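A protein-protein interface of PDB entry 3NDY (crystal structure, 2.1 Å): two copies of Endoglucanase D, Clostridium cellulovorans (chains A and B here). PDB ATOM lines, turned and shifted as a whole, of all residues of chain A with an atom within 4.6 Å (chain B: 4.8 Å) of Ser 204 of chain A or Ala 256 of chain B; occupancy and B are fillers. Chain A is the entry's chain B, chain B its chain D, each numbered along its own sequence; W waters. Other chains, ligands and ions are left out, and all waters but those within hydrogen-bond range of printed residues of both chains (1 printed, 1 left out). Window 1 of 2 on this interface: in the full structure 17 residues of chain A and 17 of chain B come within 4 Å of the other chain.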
ATOM      1  N   ALA A 202     -26.232  -4.105  27.734  1.00  0.00           N
ATOM      2  CA  ALA A 202     -25.026  -3.295  27.559  1.00  0.00           C
ATOM      3  C   ALA A 202     -25.082  -2.425  26.301  1.00  0.00           C
ATOM      4  O   ALA A 202     -24.112  -1.747  25.985  1.00  0.00           O
ATOM      5  CB  ALA A 202     -23.799  -4.189  27.513  1.00  0.00           C
ATOM      6  N   MET A 203     -26.203  -2.455  25.586  1.00  0.00           N
ATOM      7  CA  MET A 203     -26.324  -1.710  24.330  1.00  0.00           C
ATOM      8  C   MET A 203     -26.287  -0.198  24.595  1.00  0.00           C
ATOM      9  O   MET A 203     -26.613   0.258  25.707  1.00  0.00           O
ATOM     10  CB  MET A 203     -27.617  -2.081  23.601  1.00  0.00           C
ATOM     11  CG  MET A 203     -28.831  -1.340  24.140  1.00  0.00           C
ATOM     12  SD  MET A 203     -30.372  -1.648  23.239  1.00  0.00           S
ATOM     13  CE  MET A 203     -30.788  -3.274  23.822  1.00  0.00           C
ATOM     14  N   SER A 204     -25.905   0.583  23.584  1.00  0.00           N
ATOM     15  CA  SER A 204     -25.652   2.020  23.791  1.00  0.00           C
ATOM     16  C   SER A 204     -26.830   2.738  24.409  1.00  0.00           C
ATOM     17  O   SER A 204     -26.659   3.554  25.310  1.00  0.00           O
ATOM     18  CB  SER A 204     -25.282   2.716  22.482  1.00  0.00           C
ATOM     19  OG  SER A 204     -24.379   1.922  21.741  1.00  0.00           O
ATOM     20  N   THR A 205     -28.029   2.434  23.917  1.00  0.00           N
ATOM     21  CA  THR A 205     -29.230   3.115  24.384  1.00  0.00           C
ATOM     22  C   THR A 205     -29.367   3.000  25.898  1.00  0.00           C
ATOM     23  O   THR A 205     -29.612   3.989  26.589  1.00  0.00           O
ATOM     24  CB  THR A 205     -30.515   2.544  23.756  1.00  0.00           C
ATOM     25  OG1 THR A 205     -30.443   2.612  22.322  1.00  0.00           O
ATOM     26  CG2 THR A 205     -31.734   3.333  24.257  1.00  0.00           C
ATOM     27  N   THR A 206     -29.201   1.785  26.407  1.00  0.00           N
ATOM     28  CA  THR A 206     -29.454   1.521  27.816  1.00  0.00           C
ATOM     29  C   THR A 206     -28.332   1.994  28.738  1.00  0.00           C
ATOM     30  O   THR A 206     -28.603   2.528  29.811  1.00  0.00           O
ATOM     31  CB  THR A 206     -29.771   0.037  28.070  1.00  0.00           C
ATOM     32  OG1 THR A 206     -28.765  -0.776  27.456  1.00  0.00           O
ATOM     33  CG2 THR A 206     -31.128  -0.315  27.463  1.00  0.00           C
ATOM     34  N   ILE A 207     -27.078   1.797  28.343  1.00  0.00           N
ATOM     35  CA  ILE A 207     -25.975   2.282  29.177  1.00  0.00           C
ATOM     36  C   ILE A 207     -25.894   3.815  29.169  1.00  0.00           C
ATOM     37  O   ILE A 207     -25.557   4.411  30.192  1.00  0.00           O
ATOM     38  CB  ILE A 207     -24.593   1.658  28.804  1.00  0.00           C
ATOM     39  CG1 ILE A 207     -24.197   2.009  27.368  1.00  0.00           C
ATOM     40  CG2 ILE A 207     -24.606   0.131  29.028  1.00  0.00           C
ATOM     41  CD1 ILE A 207     -22.761   1.597  27.014  1.00  0.00           C
ATOM     42  N   ASN A 208     -26.200   4.444  28.028  1.00  0.00           N
ATOM     43  CA  ASN A 208     -26.211   5.910  27.927  1.00  0.00           C
ATOM     44  C   ASN A 208     -27.284   6.546  28.809  1.00  0.00           C
ATOM     45  O   ASN A 208     -27.125   7.670  29.277  1.00  0.00           O
ATOM     46  CB  ASN A 208     -26.469   6.396  26.490  1.00  0.00           C
ATOM     47  CG  ASN A 208     -25.320   6.100  25.525  1.00  0.00           C
ATOM     48  OD1 ASN A 208     -24.248   5.645  25.910  1.00  0.00           O
ATOM     49  ND2 ASN A 208     -25.559   6.378  24.251  1.00  0.00           N
ATOM     50  N   ILE B 207     -14.239   4.304  17.636  1.00  0.00           N
ATOM     51  CA  ILE B 207     -14.676   5.655  18.008  1.00  0.00           C
ATOM     52  C   ILE B 207     -14.027   6.113  19.313  1.00  0.00           C
ATOM     53  O   ILE B 207     -13.706   7.296  19.476  1.00  0.00           O
ATOM     54  CB  ILE B 207     -16.227   5.825  18.055  1.00  0.00           C
ATOM     55  CG1 ILE B 207     -16.849   5.023  19.207  1.00  0.00           C
ATOM     56  CG2 ILE B 207     -16.857   5.464  16.698  1.00  0.00           C
ATOM     57  CD1 ILE B 207     -18.363   5.176  19.305  1.00  0.00           C
ATOM     58  N   SER B 252     -29.823   2.447  18.564  1.00  0.00           N
ATOM     59  CA  SER B 252     -28.726   2.251  19.508  1.00  0.00           C
ATOM     60  C   SER B 252     -27.379   2.471  18.837  1.00  0.00           C
ATOM     61  O   SER B 252     -26.448   2.993  19.450  1.00  0.00           O
ATOM     62  CB  SER B 252     -28.796   0.858  20.134  1.00  0.00           C
ATOM     63  OG  SER B 252     -27.836   0.724  21.156  1.00  0.00           O
ATOM     64  N   GLU B 253     -27.271   2.067  17.574  1.00  0.00           N
ATOM     65  CA  GLU B 253     -26.066   2.356  16.807  1.00  0.00           C
ATOM     66  C   GLU B 253     -25.821   3.859  16.726  1.00  0.00           C
ATOM     67  O   GLU B 253     -24.702   4.315  16.932  1.00  0.00           O
ATOM     68  CB  GLU B 253     -26.133   1.744  15.400  1.00  0.00           C
ATOM     69  CG  GLU B 253     -25.985   0.227  15.397  1.00  0.00           C
ATOM     70  CD  GLU B 253     -25.825  -0.346  13.994  1.00  0.00           C
ATOM     71  OE1 GLU B 253     -24.831  -0.006  13.309  1.00  0.00           O
ATOM     72  OE2 GLU B 253     -26.694  -1.147  13.582  1.00  0.00           O
ATOM     73  N   PHE B 254     -26.863   4.632  16.421  1.00  0.00           N
ATOM     74  CA  PHE B 254     -26.702   6.084  16.378  1.00  0.00           C
ATOM     75  C   PHE B 254     -26.483   6.674  17.780  1.00  0.00           C
ATOM     76  O   PHE B 254     -25.799   7.698  17.932  1.00  0.00           O
ATOM     77  CB  PHE B 254     -27.891   6.758  15.687  1.00  0.00           C
ATOM     78  CG  PHE B 254     -28.118   6.287  14.281  1.00  0.00           C
ATOM     79  CD1 PHE B 254     -27.044   6.045  13.427  1.00  0.00           C
ATOM     80  CD2 PHE B 254     -29.404   6.090  13.803  1.00  0.00           C
ATOM     81  CE1 PHE B 254     -27.255   5.617  12.128  1.00  0.00           C
ATOM     82  CE2 PHE B 254     -29.617   5.652  12.497  1.00  0.00           C
ATOM     83  CZ  PHE B 254     -28.535   5.419  11.665  1.00  0.00           C
ATOM     84  N   ASP B 255     -27.072   6.042  18.798  1.00  0.00           N
ATOM     85  CA  ASP B 255     -26.884   6.497  20.185  1.00  0.00           C
ATOM     86  C   ASP B 255     -25.426   6.450  20.630  1.00  0.00           C
ATOM     87  O   ASP B 255     -25.002   7.278  21.430  1.00  0.00           O
ATOM     88  CB  ASP B 255     -27.742   5.692  21.162  1.00  0.00           C
ATOM     89  CG  ASP B 255     -29.218   5.967  20.985  1.00  0.00           C
ATOM     90  OD1 ASP B 255     -29.537   7.013  20.378  1.00  0.00           O
ATOM     91  OD2 ASP B 255     -30.052   5.148  21.434  1.00  0.00           O
ATOM     92  N   ALA B 256     -24.660   5.480  20.131  1.00  0.00           N
ATOM     93  CA  ALA B 256     -23.244   5.397  20.500  1.00  0.00           C
ATOM     94  C   ALA B 256     -22.515   6.628  19.960  1.00  0.00           C
ATOM     95  O   ALA B 256     -21.703   7.250  20.654  1.00  0.00           O
ATOM     96  CB  ALA B 256     -22.612   4.114  19.973  1.00  0.00           C
ATOM     97  N   VAL B 257     -22.842   6.989  18.723  1.00  0.00           N
ATOM     98  CA  VAL B 257     -22.217   8.124  18.053  1.00  0.00           C
ATOM     99  C   VAL B 257     -22.615   9.445  18.718  1.00  0.00           C
ATOM    100  O   VAL B 257     -21.787  10.307  18.958  1.00  0.00           O
ATOM    101  CB  VAL B 257     -22.594   8.129  16.567  1.00  0.00           C
ATOM    102  CG1 VAL B 257     -21.994   9.334  15.865  1.00  0.00           C
ATOM    103  CG2 VAL B 257     -22.093   6.841  15.924  1.00  0.00           C
ATOM    104  N   TYR B 258     -23.894   9.580  19.029  1.00  0.00           N
ATOM    105  CA  TYR B 258     -24.400  10.758  19.719  1.00  0.00           C
ATOM    106  C   TYR B 258     -23.719  10.978  21.083  1.00  0.00           C
ATOM    107  O   TYR B 258     -23.299  12.092  21.397  1.00  0.00           O
ATOM    108  CB  TYR B 258     -25.925  10.652  19.893  1.00  0.00           C
ATOM    109  CG  TYR B 258     -26.526  11.883  20.530  1.00  0.00           C
ATOM    110  CD1 TYR B 258     -26.766  11.935  21.897  1.00  0.00           C
ATOM    111  CD2 TYR B 258     -26.802  13.013  19.766  1.00  0.00           C
ATOM    112  CE1 TYR B 258     -27.295  13.078  22.489  1.00  0.00           C
ATOM    113  CE2 TYR B 258     -27.324  14.148  20.339  1.00  0.00           C
ATOM    114  CZ  TYR B 258     -27.572  14.177  21.702  1.00  0.00           C
ATOM    115  OH  TYR B 258     -28.089  15.312  22.274  1.00  0.00           O
ATOM    116  N   ASN B 259     -23.619   9.919  21.886  1.00  0.00           N
ATOM    117  CA  ASN B 259     -23.035  10.052  23.212  1.00  0.00           C
ATOM    118  C   ASN B 259     -21.519  10.307  23.198  1.00  0.00           C
ATOM    119  O   ASN B 259     -21.021  11.080  24.008  1.00  0.00           O
ATOM    120  CB  ASN B 259     -23.398   8.851  24.089  1.00  0.00           C
ATOM    121  CG  ASN B 259     -24.154   9.253  25.348  1.00  0.00           C
ATOM    122  OD1 ASN B 259     -23.614   9.185  26.449  1.00  0.00           O
ATOM    123  ND2 ASN B 259     -25.405   9.677  25.190  1.00  0.00           N
ATOM    124  N   LYS B 260     -20.799   9.678  22.277  1.00  0.00           N
ATOM    125  CA  LYS B 260     -19.359   9.881  22.178  1.00  0.00           C
ATOM    126  C   LYS B 260     -18.986  11.227  21.546  1.00  0.00           C
ATOM    127  O   LYS B 260     -18.056  11.889  21.991  1.00  0.00           O
ATOM    128  CB  LYS B 260     -18.711   8.724  21.413  1.00  0.00           C
ATOM    129  CG  LYS B 260     -17.255   8.940  21.051  1.00  0.00           C
ATOM    130  CD  LYS B 260     -16.404   9.241  22.277  1.00  0.00           C
ATOM    131  CE  LYS B 260     -16.276   8.029  23.177  1.00  0.00           C
ATOM    132  NZ  LYS B 260     -15.233   8.222  24.226  1.00  0.00           N
HETATM  133  O   HOH W   1     -28.194   8.138  24.041  1.00  0.00           O
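O of Met 203 of chain A is in hydrogen-bond range of OG1 of Thr 206 of chain A (3.0 Å).
The side-chain amide nitrogen (ND2) of Asn 208 of chain A sits close to the backbone carbonyl oxygen (O) of Ser 204 of chain A (3.2 Å).
The side-chain amide nitrogen of Asn 259 of chain B lies close to the side-chain amide nitrogen of Asn 208 of chain A (3.4 Å).
N of Thr 205 of chain A lies within hydrogen-bond range of OG of Ser 252 of chain B (3.3 Å).
The backbone NH of Ser 204 of chain A sits at hydrogen-bond distance from the side-chain hydroxyl of Ser 252 of chain B.
The side-chain carboxylate (OD2) of Asp 255 of chain B lies within hydrogen-bond range of the side-chain hydroxyl (OG1) of Thr 205 of chain A (2.7 Å).
The backbone carbonyl oxygen (O) of Asp 255 of chain B is in hydrogen-bond range of the side-chain amide nitrogen (ND2) of Asn 208 of chain A, at 3.0 Å.
1 position is printed for both chains.
Hydrophobic or aromatic side chains of chain A that line the printed part of chain B: Met 203.
Printed residues of chain B that touch a printed residue of chain A: Ser 252, Asp 255, Ala 256 and Asn 259.
Hydrophobic or aromatic side chains of chain B that line the printed part of chain A: Ala 256.
Among the printed residues, 7 pairs touch across the chains.
Among the printed residues, no Asp or Glu carboxylate lies within 4 Å of a Lys or Arg side-chain nitrogen of the other chain.
Water W1 bridges ND2 of Asn 208 of chain A (3.2 Å) and ND2 of Asn 259 of chain B (3.4 Å).
Of the printed residues of chain B, Met 203 of chain A touches Ser 252.
Of chain B, only Ser 252 (3.1 Å) and Ala 256 (3.3 Å) come within 4 Å of Ser 204 of chain A.
Printed residues of chain B within 4 Å of Asn 208 of chain A: Asp 255 (3.0 Å) and Asn 259 (3.3 Å).
Of the printed residues of chain A, Ser 252 of chain B touches Met 203 (3.7 Å), Ser 204 (3.1 Å) and Thr 205 (3.3 Å).
Glu 253 of chain B touches none of the printed residues of chain A.
Of the printed residues of chain A, Asp 255 of chain B touches Thr 205 and Asn 208.
Ala 256 of chain B touches just one residue of chain A: Ser 204 (3.3 Å).
Printed residues of chain A within 4 Å of Asn 259 of chain B: Asn 208.
Lys 260 of chain B touches none of the printed residues of chain A.
The nearest residue of chain B that does not touch Ser 204 of chain A is Asp 255 of chain B (4.1 Å).
The nearest residue of chain A that does not touch Ala 256 of chain B is Asn 208 of chain A (4.3 Å).
Among the printed residues, pairs that only touch across the chains: Met 203 of chain A with Ser 252 of chain B and Ser 204 of chain A with Ala 256 of chain B.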
